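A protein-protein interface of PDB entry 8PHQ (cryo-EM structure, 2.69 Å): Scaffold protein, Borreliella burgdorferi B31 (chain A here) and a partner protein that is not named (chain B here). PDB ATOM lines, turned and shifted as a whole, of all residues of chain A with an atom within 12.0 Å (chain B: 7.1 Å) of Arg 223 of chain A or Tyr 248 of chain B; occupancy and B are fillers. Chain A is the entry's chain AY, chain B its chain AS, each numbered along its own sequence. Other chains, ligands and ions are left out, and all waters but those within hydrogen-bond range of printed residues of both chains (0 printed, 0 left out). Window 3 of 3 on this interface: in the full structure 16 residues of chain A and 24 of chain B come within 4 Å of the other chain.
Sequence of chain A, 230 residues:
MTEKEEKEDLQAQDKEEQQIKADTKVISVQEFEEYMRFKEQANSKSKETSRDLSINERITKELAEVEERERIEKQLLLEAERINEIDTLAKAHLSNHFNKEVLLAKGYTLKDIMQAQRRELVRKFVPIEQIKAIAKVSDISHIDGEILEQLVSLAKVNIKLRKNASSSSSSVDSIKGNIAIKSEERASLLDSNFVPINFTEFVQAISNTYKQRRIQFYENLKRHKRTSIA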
ATOM      1  N   ARG A 214       1.000  -9.726  25.843  1.00  0.00           N
ATOM      2  CA  ARG A 214       0.907 -10.769  24.822  1.00  0.00           C
ATOM      3  C   ARG A 214       2.237 -11.500  24.654  1.00  0.00           C
ATOM      4  O   ARG A 214       2.274 -12.739  24.570  1.00  0.00           O
ATOM      5  CB  ARG A 214       0.467 -10.160  23.494  1.00  0.00           C
ATOM      6  CG  ARG A 214       0.217 -11.171  22.393  1.00  0.00           C
ATOM      7  CD  ARG A 214       0.594 -10.578  21.057  1.00  0.00           C
ATOM      8  NE  ARG A 214       0.056  -9.233  20.909  1.00  0.00           N
ATOM      9  CZ  ARG A 214       0.337  -8.418  19.902  1.00  0.00           C
ATOM     10  NH1 ARG A 214       1.173  -8.771  18.940  1.00  0.00           N
ATOM     11  NH2 ARG A 214      -0.225  -7.214  19.868  1.00  0.00           N
ATOM     12  N   ILE A 215       3.338 -10.747  24.606  1.00  0.00           N
ATOM     13  CA  ILE A 215       4.653 -11.375  24.471  1.00  0.00           C
ATOM     14  C   ILE A 215       4.946 -12.270  25.670  1.00  0.00           C
ATOM     15  O   ILE A 215       5.467 -13.382  25.521  1.00  0.00           O
ATOM     16  CB  ILE A 215       5.749 -10.311  24.277  1.00  0.00           C
ATOM     17  CG1 ILE A 215       5.406  -9.396  23.101  1.00  0.00           C
ATOM     18  CG2 ILE A 215       7.103 -10.969  24.068  1.00  0.00           C
ATOM     19  CD1 ILE A 215       6.366  -8.243  22.922  1.00  0.00           C
ATOM     20  N   GLN A 216       4.617 -11.805  26.876  1.00  0.00           N
ATOM     21  CA  GLN A 216       4.847 -12.615  28.068  1.00  0.00           C
ATOM     22  C   GLN A 216       3.998 -13.882  28.052  1.00  0.00           C
ATOM     23  O   GLN A 216       4.461 -14.957  28.457  1.00  0.00           O
ATOM     24  CB  GLN A 216       4.567 -11.790  29.324  1.00  0.00           C
ATOM     25  CG  GLN A 216       4.714 -12.565  30.619  1.00  0.00           C
ATOM     26  CD  GLN A 216       4.689 -11.668  31.840  1.00  0.00           C
ATOM     27  OE1 GLN A 216       4.591 -10.447  31.725  1.00  0.00           O
ATOM     28  NE2 GLN A 216       4.784 -12.272  33.019  1.00  0.00           N
ATOM     29  N   PHE A 217       2.749 -13.777  27.588  1.00  0.00           N
ATOM     30  CA  PHE A 217       1.893 -14.956  27.504  1.00  0.00           C
ATOM     31  C   PHE A 217       2.492 -15.990  26.564  1.00  0.00           C
ATOM     32  O   PHE A 217       2.508 -17.187  26.870  1.00  0.00           O
ATOM     33  CB  PHE A 217       0.494 -14.574  27.027  1.00  0.00           C
ATOM     34  CG  PHE A 217      -0.337 -15.755  26.605  1.00  0.00           C
ATOM     35  CD1 PHE A 217      -0.822 -16.642  27.548  1.00  0.00           C
ATOM     36  CD2 PHE A 217      -0.591 -16.005  25.269  1.00  0.00           C
ATOM     37  CE1 PHE A 217      -1.577 -17.734  27.170  1.00  0.00           C
ATOM     38  CE2 PHE A 217      -1.339 -17.104  24.887  1.00  0.00           C
ATOM     39  CZ  PHE A 217      -1.834 -17.964  25.839  1.00  0.00           C
ATOM     40  N   TYR A 218       2.982 -15.547  25.403  1.00  0.00           N
ATOM     41  CA  TYR A 218       3.599 -16.501  24.486  1.00  0.00           C
ATOM     42  C   TYR A 218       4.925 -17.036  25.014  1.00  0.00           C
ATOM     43  O   TYR A 218       5.320 -18.151  24.659  1.00  0.00           O
ATOM     44  CB  TYR A 218       3.782 -15.884  23.102  1.00  0.00           C
ATOM     45  CG  TYR A 218       2.503 -15.839  22.300  1.00  0.00           C
ATOM     46  CD1 TYR A 218       1.810 -17.006  22.014  1.00  0.00           C
ATOM     47  CD2 TYR A 218       1.996 -14.641  21.820  1.00  0.00           C
ATOM     48  CE1 TYR A 218       0.644 -16.983  21.280  1.00  0.00           C
ATOM     49  CE2 TYR A 218       0.829 -14.609  21.083  1.00  0.00           C
ATOM     50  CZ  TYR A 218       0.158 -15.783  20.817  1.00  0.00           C
ATOM     51  OH  TYR A 218      -1.005 -15.755  20.084  1.00  0.00           O
ATOM     52  N   GLU A 219       5.627 -16.272  25.853  1.00  0.00           N
ATOM     53  CA  GLU A 219       6.841 -16.809  26.461  1.00  0.00           C
ATOM     54  C   GLU A 219       6.530 -17.850  27.530  1.00  0.00           C
ATOM     55  O   GLU A 219       7.342 -18.750  27.769  1.00  0.00           O
ATOM     56  CB  GLU A 219       7.689 -15.685  27.054  1.00  0.00           C
ATOM     57  CG  GLU A 219       8.377 -14.818  26.018  1.00  0.00           C
ATOM     58  CD  GLU A 219       8.958 -13.550  26.608  1.00  0.00           C
ATOM     59  OE1 GLU A 219       8.779 -13.319  27.822  1.00  0.00           O
ATOM     60  OE2 GLU A 219       9.601 -12.786  25.858  1.00  0.00           O
ATOM     61  N   ASN A 220       5.375 -17.746  28.183  1.00  0.00           N
ATOM     62  CA  ASN A 220       4.998 -18.704  29.217  1.00  0.00           C
ATOM     63  C   ASN A 220       4.070 -19.805  28.717  1.00  0.00           C
ATOM     64  O   ASN A 220       3.714 -20.694  29.495  1.00  0.00           O
ATOM     65  CB  ASN A 220       4.342 -17.984  30.399  1.00  0.00           C
ATOM     66  CG  ASN A 220       5.221 -16.898  30.979  1.00  0.00           C
ATOM     67  OD1 ASN A 220       6.337 -16.672  30.513  1.00  0.00           O
ATOM     68  ND2 ASN A 220       4.725 -16.223  32.008  1.00  0.00           N
ATOM     69  N   LEU A 221       3.671 -19.772  27.449  1.00  0.00           N
ATOM     70  CA  LEU A 221       2.735 -20.758  26.927  1.00  0.00           C
ATOM     71  C   LEU A 221       3.447 -22.069  26.618  1.00  0.00           C
ATOM     72  O   LEU A 221       4.499 -22.078  25.973  1.00  0.00           O
ATOM     73  CB  LEU A 221       2.046 -20.229  25.669  1.00  0.00           C
ATOM     74  CG  LEU A 221       1.085 -21.199  24.977  1.00  0.00           C
ATOM     75  CD1 LEU A 221      -0.096 -21.523  25.877  1.00  0.00           C
ATOM     76  CD2 LEU A 221       0.611 -20.637  23.648  1.00  0.00           C
ATOM     77  N   LYS A 222       2.872 -23.174  27.086  1.00  0.00           N
ATOM     78  CA  LYS A 222       3.341 -24.511  26.757  1.00  0.00           C
ATOM     79  C   LYS A 222       2.191 -25.322  26.177  1.00  0.00           C
ATOM     80  O   LYS A 222       1.051 -25.222  26.641  1.00  0.00           O
ATOM     81  CB  LYS A 222       3.930 -25.223  27.983  1.00  0.00           C
ATOM     82  CG  LYS A 222       2.938 -25.504  29.097  1.00  0.00           C
ATOM     83  CD  LYS A 222       3.604 -26.240  30.249  1.00  0.00           C
ATOM     84  CE  LYS A 222       4.524 -25.325  31.036  1.00  0.00           C
ATOM     85  NZ  LYS A 222       5.076 -26.007  32.239  1.00  0.00           N
ATOM     86  N   ARG A 223       2.491 -26.107  25.149  1.00  0.00           N
ATOM     87  CA  ARG A 223       1.474 -26.903  24.475  1.00  0.00           C
ATOM     88  C   ARG A 223       1.786 -28.394  24.573  1.00  0.00           C
ATOM     89  O   ARG A 223       1.486 -29.036  25.580  1.00  0.00           O
ATOM     90  CB  ARG A 223       1.359 -26.485  23.009  1.00  0.00           C
ATOM     91  CG  ARG A 223       1.046 -25.012  22.791  1.00  0.00           C
ATOM     92  CD  ARG A 223       1.255 -24.633  21.331  1.00  0.00           C
ATOM     93  NE  ARG A 223       0.780 -23.294  20.999  1.00  0.00           N
ATOM     94  CZ  ARG A 223      -0.492 -22.919  21.000  1.00  0.00           C
ATOM     95  NH1 ARG A 223      -1.464 -23.763  21.304  1.00  0.00           N
ATOM     96  NH2 ARG A 223      -0.798 -21.666  20.675  1.00  0.00           N
ATOM     97  N   TYR B  26      -5.434 -15.693  21.959  1.00  0.00           N
ATOM     98  CA  TYR B  26      -3.998 -15.849  21.781  1.00  0.00           C
ATOM     99  C   TYR B  26      -3.582 -17.310  21.687  1.00  0.00           C
ATOM    100  O   TYR B  26      -2.487 -17.599  21.194  1.00  0.00           O
ATOM    101  CB  TYR B  26      -3.258 -15.171  22.933  1.00  0.00           C
ATOM    102  CG  TYR B  26      -3.316 -13.661  22.919  1.00  0.00           C
ATOM    103  CD1 TYR B  26      -3.865 -12.975  21.847  1.00  0.00           C
ATOM    104  CD2 TYR B  26      -2.833 -12.924  23.990  1.00  0.00           C
ATOM    105  CE1 TYR B  26      -3.919 -11.598  21.835  1.00  0.00           C
ATOM    106  CE2 TYR B  26      -2.887 -11.548  23.989  1.00  0.00           C
ATOM    107  CZ  TYR B  26      -3.431 -10.890  22.910  1.00  0.00           C
ATOM    108  OH  TYR B  26      -3.484  -9.516  22.904  1.00  0.00           O
ATOM    109  N   LYS B  27      -4.423 -18.233  22.151  1.00  0.00           N
ATOM    110  CA  LYS B  27      -4.121 -19.654  22.074  1.00  0.00           C
ATOM    111  C   LYS B  27      -4.358 -20.239  20.689  1.00  0.00           C
ATOM    112  O   LYS B  27      -3.895 -21.351  20.420  1.00  0.00           O
ATOM    113  CB  LYS B  27      -4.954 -20.423  23.101  1.00  0.00           C
ATOM    114  CG  LYS B  27      -4.830 -19.891  24.517  1.00  0.00           C
ATOM    115  CD  LYS B  27      -5.800 -20.585  25.459  1.00  0.00           C
ATOM    116  CE  LYS B  27      -5.640 -22.093  25.405  1.00  0.00           C
ATOM    117  NZ  LYS B  27      -6.661 -22.783  26.240  1.00  0.00           N
ATOM    118  N   TRP B  28      -5.061 -19.527  19.813  1.00  0.00           N
ATOM    119  CA  TRP B  28      -5.341 -20.011  18.470  1.00  0.00           C
ATOM    120  C   TRP B  28      -4.309 -19.559  17.447  1.00  0.00           C
ATOM    121  O   TRP B  28      -4.449 -19.884  16.264  1.00  0.00           O
ATOM    122  CB  TRP B  28      -6.732 -19.552  18.020  1.00  0.00           C
ATOM    123  CG  TRP B  28      -7.825 -19.872  18.985  1.00  0.00           C
ATOM    124  CD1 TRP B  28      -7.954 -21.005  19.730  1.00  0.00           C
ATOM    125  CD2 TRP B  28      -8.960 -19.058  19.292  1.00  0.00           C
ATOM    126  NE1 TRP B  28      -9.093 -20.942  20.494  1.00  0.00           N
ATOM    127  CE2 TRP B  28      -9.730 -19.756  20.241  1.00  0.00           C
ATOM    128  CE3 TRP B  28      -9.400 -17.804  18.859  1.00  0.00           C
ATOM    129  CZ2 TRP B  28     -10.913 -19.243  20.766  1.00  0.00           C
ATOM    130  CZ3 TRP B  28     -10.573 -17.296  19.381  1.00  0.00           C
ATOM    131  CH2 TRP B  28     -11.316 -18.014  20.325  1.00  0.00           C
ATOM    132  N   PHE B  29      -3.284 -18.821  17.865  1.00  0.00           N
ATOM    133  CA  PHE B  29      -2.288 -18.291  16.949  1.00  0.00           C
ATOM    134  C   PHE B  29      -0.900 -18.493  17.536  1.00  0.00           C
ATOM    135  O   PHE B  29      -0.728 -18.607  18.751  1.00  0.00           O
ATOM    136  CB  PHE B  29      -2.525 -16.803  16.664  1.00  0.00           C
ATOM    137  CG  PHE B  29      -3.794 -16.523  15.915  1.00  0.00           C
ATOM    138  CD1 PHE B  29      -3.945 -16.932  14.603  1.00  0.00           C
ATOM    139  CD2 PHE B  29      -4.842 -15.861  16.529  1.00  0.00           C
ATOM    140  CE1 PHE B  29      -5.112 -16.677  13.914  1.00  0.00           C
ATOM    141  CE2 PHE B  29      -6.012 -15.605  15.845  1.00  0.00           C
ATOM    142  CZ  PHE B  29      -6.146 -16.013  14.535  1.00  0.00           C
ATOM    143  N   SER B  30       0.090 -18.541  16.655  1.00  0.00           N
ATOM    144  CA  SER B  30       1.484 -18.575  17.064  1.00  0.00           C
ATOM    145  C   SER B  30       1.997 -17.156  17.277  1.00  0.00           C
ATOM    146  O   SER B  30       1.410 -16.194  16.776  1.00  0.00           O
ATOM    147  CB  SER B  30       2.322 -19.293  16.010  1.00  0.00           C
ATOM    148  OG  SER B  30       2.449 -18.516  14.836  1.00  0.00           O
ATOM    149  N   PRO B  31       3.086 -16.990  18.037  1.00  0.00           N
ATOM    150  CA  PRO B  31       3.586 -15.627  18.297  1.00  0.00           C
ATOM    151  C   PRO B  31       3.918 -14.843  17.039  1.00  0.00           C
ATOM    152  O   PRO B  31       3.716 -13.624  17.004  1.00  0.00           O
ATOM    153  CB  PRO B  31       4.836 -15.878  19.149  1.00  0.00           C
ATOM    154  CG  PRO B  31       4.576 -17.175  19.814  1.00  0.00           C
ATOM    155  CD  PRO B  31       3.821 -18.000  18.817  1.00  0.00           C
ATOM    156  N   PRO B 200       3.128 -26.529  12.273  1.00  0.00           N
ATOM    157  CA  PRO B 200       2.158 -27.035  13.248  1.00  0.00           C
ATOM    158  C   PRO B 200       0.737 -26.707  12.820  1.00  0.00           C
ATOM    159  O   PRO B 200       0.475 -25.683  12.187  1.00  0.00           O
ATOM    160  CB  PRO B 200       2.537 -26.302  14.540  1.00  0.00           C
ATOM    161  CG  PRO B 200       3.965 -25.927  14.353  1.00  0.00           C
ATOM    162  CD  PRO B 200       4.109 -25.623  12.894  1.00  0.00           C
ATOM    163  N   MET B 201      -0.190 -27.593  13.173  1.00  0.00           N
ATOM    164  CA  MET B 201      -1.580 -27.457  12.769  1.00  0.00           C
ATOM    165  C   MET B 201      -2.467 -27.316  13.997  1.00  0.00           C
ATOM    166  O   MET B 201      -2.160 -27.850  15.068  1.00  0.00           O
ATOM    167  CB  MET B 201      -2.033 -28.655  11.930  1.00  0.00           C
ATOM    168  CG  MET B 201      -1.298 -28.788  10.606  1.00  0.00           C
ATOM    169  SD  MET B 201      -1.897 -27.722   9.282  1.00  0.00           S
ATOM    170  CE  MET B 201      -3.657 -28.005   9.376  1.00  0.00           C
ATOM    171  N   MET B 202      -3.567 -26.583  13.840  1.00  0.00           N
ATOM    172  CA  MET B 202      -4.497 -26.316  14.924  1.00  0.00           C
ATOM    173  C   MET B 202      -5.888 -26.793  14.535  1.00  0.00           C
ATOM    174  O   MET B 202      -6.346 -26.564  13.406  1.00  0.00           O
ATOM    175  CB  MET B 202      -4.525 -24.822  15.270  1.00  0.00           C
ATOM    176  CG  MET B 202      -5.700 -24.386  16.135  1.00  0.00           C
ATOM    177  SD  MET B 202      -5.676 -25.104  17.787  1.00  0.00           S
ATOM    178  CE  MET B 202      -4.377 -24.144  18.554  1.00  0.00           C
ATOM    179  N   VAL B 203      -6.544 -27.462  15.483  1.00  0.00           N
ATOM    180  CA  VAL B 203      -7.899 -27.973  15.339  1.00  0.00           C
ATOM    181  C   VAL B 203      -8.735 -27.386  16.466  1.00  0.00           C
ATOM    182  O   VAL B 203      -8.311 -27.396  17.625  1.00  0.00           O
ATOM    183  CB  VAL B 203      -7.934 -29.511  15.390  1.00  0.00           C
ATOM    184  CG1 VAL B 203      -9.346 -30.022  15.165  1.00  0.00           C
ATOM    185  CG2 VAL B 203      -6.973 -30.099  14.378  1.00  0.00           C
ATOM    186  N   ILE B 204      -9.903 -26.854  16.120  1.00  0.00           N
ATOM    187  CA  ILE B 204     -10.852 -26.311  17.084  1.00  0.00           C
ATOM    188  C   ILE B 204     -12.176 -27.038  16.906  1.00  0.00           C
ATOM    189  O   ILE B 204     -12.703 -27.111  15.788  1.00  0.00           O
ATOM    190  CB  ILE B 204     -11.029 -24.792  16.918  1.00  0.00           C
ATOM    191  CG1 ILE B 204      -9.667 -24.099  16.891  1.00  0.00           C
ATOM    192  CG2 ILE B 204     -11.888 -24.236  18.036  1.00  0.00           C
ATOM    193  CD1 ILE B 204      -9.749 -22.599  16.795  1.00  0.00           C
ATOM    194  N   ILE B 235      -5.444 -37.095  14.507  1.00  0.00           N
ATOM    195  CA  ILE B 235      -4.100 -36.543  14.655  1.00  0.00           C
ATOM    196  C   ILE B 235      -3.141 -37.200  13.673  1.00  0.00           C
ATOM    197  O   ILE B 235      -2.298 -36.530  13.069  1.00  0.00           O
ATOM    198  CB  ILE B 235      -3.610 -36.679  16.108  1.00  0.00           C
ATOM    199  CG1 ILE B 235      -4.530 -35.907  17.053  1.00  0.00           C
ATOM    200  CG2 ILE B 235      -2.182 -36.184  16.243  1.00  0.00           C
ATOM    201  CD1 ILE B 235      -4.177 -36.060  18.511  1.00  0.00           C
ATOM    202  N   ILE B 238      -3.787 -35.737  10.147  1.00  0.00           N
ATOM    203  CA  ILE B 238      -3.223 -34.399   9.975  1.00  0.00           C
ATOM    204  C   ILE B 238      -1.697 -34.447   9.944  1.00  0.00           C
ATOM    205  O   ILE B 238      -1.049 -33.677   9.218  1.00  0.00           O
ATOM    206  CB  ILE B 238      -3.747 -33.457  11.071  1.00  0.00           C
ATOM    207  CG1 ILE B 238      -5.274 -33.438  11.048  1.00  0.00           C
ATOM    208  CG2 ILE B 238      -3.199 -32.057  10.878  1.00  0.00           C
ATOM    209  CD1 ILE B 238      -5.883 -32.599  12.128  1.00  0.00           C
ATOM    210  N   ASN B 242       1.175 -32.567   7.526  1.00  0.00           N
ATOM    211  CA  ASN B 242       1.976 -31.462   8.044  1.00  0.00           C
ATOM    212  C   ASN B 242       3.414 -31.874   8.363  1.00  0.00           C
ATOM    213  O   ASN B 242       4.055 -31.249   9.214  1.00  0.00           O
ATOM    214  CB  ASN B 242       1.314 -30.830   9.271  1.00  0.00           C
ATOM    215  CG  ASN B 242       1.380 -31.704  10.506  1.00  0.00           C
ATOM    216  OD1 ASN B 242       1.823 -32.845  10.459  1.00  0.00           O
ATOM    217  ND2 ASN B 242       0.947 -31.154  11.631  1.00  0.00           N
ATOM    218  N   GLU B 245       4.546 -32.966  12.214  1.00  0.00           N
ATOM    219  CA  GLU B 245       4.755 -31.945  13.230  1.00  0.00           C
ATOM    220  C   GLU B 245       3.531 -31.841  14.132  1.00  0.00           C
ATOM    221  O   GLU B 245       2.546 -32.566  13.975  1.00  0.00           O
ATOM    222  CB  GLU B 245       5.104 -30.601  12.592  1.00  0.00           C
ATOM    223  CG  GLU B 245       6.458 -30.602  11.908  1.00  0.00           C
ATOM    224  CD  GLU B 245       6.801 -29.268  11.291  1.00  0.00           C
ATOM    225  OE1 GLU B 245       5.933 -28.377  11.297  1.00  0.00           O
ATOM    226  OE2 GLU B 245       7.940 -29.106  10.806  1.00  0.00           O
ATOM    227  N   ASP B 246       3.608 -30.921  15.091  1.00  0.00           N
ATOM    228  CA  ASP B 246       2.639 -30.873  16.177  1.00  0.00           C
ATOM    229  C   ASP B 246       1.243 -30.538  15.667  1.00  0.00           C
ATOM    230  O   ASP B 246       1.064 -29.687  14.790  1.00  0.00           O
ATOM    231  CB  ASP B 246       3.068 -29.846  17.223  1.00  0.00           C
ATOM    232  CG  ASP B 246       4.406 -30.180  17.854  1.00  0.00           C
ATOM    233  OD1 ASP B 246       4.531 -31.274  18.443  1.00  0.00           O
ATOM    234  OD2 ASP B 246       5.330 -29.346  17.763  1.00  0.00           O
ATOM    235  N   VAL B 247       0.250 -31.223  16.228  1.00  0.00           N
ATOM    236  CA  VAL B 247      -1.158 -30.970  15.951  1.00  0.00           C
ATOM    237  C   VAL B 247      -1.825 -30.697  17.290  1.00  0.00           C
ATOM    238  O   VAL B 247      -1.924 -31.596  18.134  1.00  0.00           O
ATOM    239  CB  VAL B 247      -1.833 -32.147  15.237  1.00  0.00           C
ATOM    240  CG1 VAL B 247      -3.305 -31.853  15.012  1.00  0.00           C
ATOM    241  CG2 VAL B 247      -1.134 -32.441  13.925  1.00  0.00           C
ATOM    242  N   TYR B 248      -2.287 -29.468  17.487  1.00  0.00           N
ATOM    243  CA  TYR B 248      -2.928 -29.067  18.730  1.00  0.00           C
ATOM    244  C   TYR B 248      -4.440 -29.120  18.572  1.00  0.00           C
ATOM    245  O   TYR B 248      -4.974 -28.774  17.516  1.00  0.00           O
ATOM    246  CB  TYR B 248      -2.492 -27.663  19.145  1.00  0.00           C
ATOM    247  CG  TYR B 248      -1.000 -27.447  19.085  1.00  0.00           C
ATOM    248  CD1 TYR B 248      -0.140 -28.198  19.873  1.00  0.00           C
ATOM    249  CD2 TYR B 248      -0.449 -26.490  18.246  1.00  0.00           C
ATOM    250  CE1 TYR B 248       1.224 -28.005  19.824  1.00  0.00           C
ATOM    251  CE2 TYR B 248       0.913 -26.288  18.191  1.00  0.00           C
ATOM    252  CZ  TYR B 248       1.746 -27.050  18.982  1.00  0.00           C
ATOM    253  OH  TYR B 248       3.106 -26.854  18.934  1.00  0.00           O
ATOM    254  N   ILE B 249      -5.120 -29.578  19.618  1.00  0.00           N
ATOM    255  CA  ILE B 249      -6.573 -29.702  19.633  1.00  0.00           C
ATOM    256  C   ILE B 249      -7.116 -28.827  20.751  1.00  0.00           C
ATOM    257  O   ILE B 249      -6.639 -28.898  21.889  1.00  0.00           O
ATOM    258  CB  ILE B 249      -7.018 -31.163  19.815  1.00  0.00           C
ATOM    259  CG1 ILE B 249      -6.476 -32.024  18.674  1.00  0.00           C
ATOM    260  CG2 ILE B 249      -8.531 -31.256  19.875  1.00  0.00           C
ATOM    261  CD1 ILE B 249      -7.029 -33.425  18.656  1.00  0.00           C
ATOM    262  N   GLU B 250      -8.109 -28.003  20.426  1.00  0.00           N
ATOM    263  CA  GLU B 250      -8.722 -27.098  21.381  1.00  0.00           C
ATOM    264  C   GLU B 250     -10.236 -27.203  21.284  1.00  0.00           C
ATOM    265  O   GLU B 250     -10.790 -27.527  20.228  1.00  0.00           O
ATOM    266  CB  GLU B 250      -8.279 -25.651  21.141  1.00  0.00           C
ATOM    267  CG  GLU B 250      -6.857 -25.361  21.591  1.00  0.00           C
ATOM    268  CD  GLU B 250      -6.766 -25.029  23.068  1.00  0.00           C
ATOM    269  OE1 GLU B 250      -7.819 -24.976  23.735  1.00  0.00           O
ATOM    270  OE2 GLU B 250      -5.638 -24.824  23.562  1.00  0.00           O
ATOM    271  N   LEU B 260     -12.807 -26.702  12.886  1.00  0.00           N
ATOM    272  CA  LEU B 260     -11.903 -25.788  12.203  1.00  0.00           C
ATOM    273  C   LEU B 260     -10.504 -26.381  12.204  1.00  0.00           C
ATOM    274  O   LEU B 260      -9.993 -26.756  13.261  1.00  0.00           O
ATOM    275  CB  LEU B 260     -11.886 -24.419  12.884  1.00  0.00           C
ATOM    276  CG  LEU B 260     -12.861 -23.355  12.391  1.00  0.00           C
ATOM    277  CD1 LEU B 260     -12.656 -22.064  13.165  1.00  0.00           C
ATOM    278  CD2 LEU B 260     -12.674 -23.128  10.905  1.00  0.00           C
ATOM    279  N   LEU B 264      -0.679 -23.160  11.764  1.00  0.00           N
ATOM    280  CA  LEU B 264      -0.115 -22.097  12.596  1.00  0.00           C
ATOM    281  C   LEU B 264       1.137 -21.504  11.960  1.00  0.00           C
ATOM    282  O   LEU B 264       2.199 -21.441  12.577  1.00  0.00           O
ATOM    283  CB  LEU B 264       0.182 -22.633  13.991  1.00  0.00           C
ATOM    284  CG  LEU B 264      -1.016 -23.114  14.806  1.00  0.00           C
ATOM    285  CD1 LEU B 264      -0.597 -23.438  16.227  1.00  0.00           C
ATOM    286  CD2 LEU B 264      -2.114 -22.069  14.799  1.00  0.00           C
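Of the printed residues of chain B, Arg 223 of chain A touches Lys 27 (3.1 Å), Phe 29 (3.6 Å) and Tyr 248 (3.4 Å). Of the printed residues of chain A, Tyr 248 of chain B touches Arg 223. Of chain A, only Phe 217 (3.8 Å) and Arg 223 (3.1 Å) come within 4 Å of Lys 27 of chain B. Ser 30 of chain B touches none of the printed residues of chain A. No residue of chain A comes within 4 Å of Pro 200 of chain B. Met 202 of chain B touches none of the printed residues of chain A. No residue of chain A comes within 4 Å of Asp 246 of chain B. No residue of chain A comes within 4 Å of Ile 249 of chain B. No residue of chain A comes within 4 Å of Leu 264 of chain B. Printed residues of chain A within 4 Å of Tyr 26 of chain B: Arg 214 (3.5 Å), Phe 217 (3.4 Å) and Tyr 218 (2.6 Å). Printed residues of chain A within 4 Å of Phe 29 of chain B: Tyr 218 (3.2 Å) and Arg 223 (3.6 Å). Printed residues of chain B within 4 Å of Tyr 218 of chain A: Tyr 26 (2.6 Å), Phe 29 (3.2 Å) and Pro 31 (3.5 Å). Of the printed residues of chain A, Pro 31 of chain B touches Tyr 218. Met 201 of chain B touches none of the printed residues of chain A. The nearest residue of chain B that does not touch Arg 223 of chain A is Met 202 of chain B (4.02 Å).
The side-chain hydroxyl of Tyr 218 of chain A is in hydrogen-bond range of the backbone carbonyl oxygen of Tyr 26 of chain B, at 2.6 Å. NH2 of Arg 223 of chain A sits at hydrogen-bond distance from O of Lys 27 of chain B (3.1 Å). The side-chain hydroxyl (OH) of Tyr 218 of chain A is in hydrogen-bond range of the backbone carbonyl oxygen (O) of Phe 29 of chain B (3.2 Å).
Hydrophobic or aromatic side chains of chain B within 4 Å of the printed part of chain A: Tyr 26, Phe 29, Pro 31 and Tyr 248. Of the 10 printed residues of chain A, 4 touch a printed residue of chain B. Among the printed residues, 9 pairs touch across the chains.
Among the printed residues, pairs that only touch across the chains: Phe 217 of chain A with Tyr 26 of chain B (3.4 Å), Arg 223 of chain A with Tyr 248 of chain B (3.4 Å), Tyr 218 of chain A with Pro 31 of chain B (3.5 Å), Arg 214 of chain A with Tyr 26 of chain B (3.5 Å), Arg 223 of chain A with Phe 29 of chain B (3.6 Å) and Phe 217 of chain A with Lys 27 of chain B (3.8 Å).
The side-chain carboxylate (OE2) of Glu 250 of chain B is in salt-bridge range of the side-chain amino group (NZ) of Lys 27 of chain B (3.5 Å). The backbone carbonyl oxygen of Met 201 of chain B sits at hydrogen-bond distance from the backbone NH of Tyr 248 of chain B (2.9 Å). The backbone NH (N) of Val 203 of chain B sits at hydrogen-bond distance from the backbone carbonyl oxygen (O) of Tyr 248 of chain B, 2.9 Å away.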
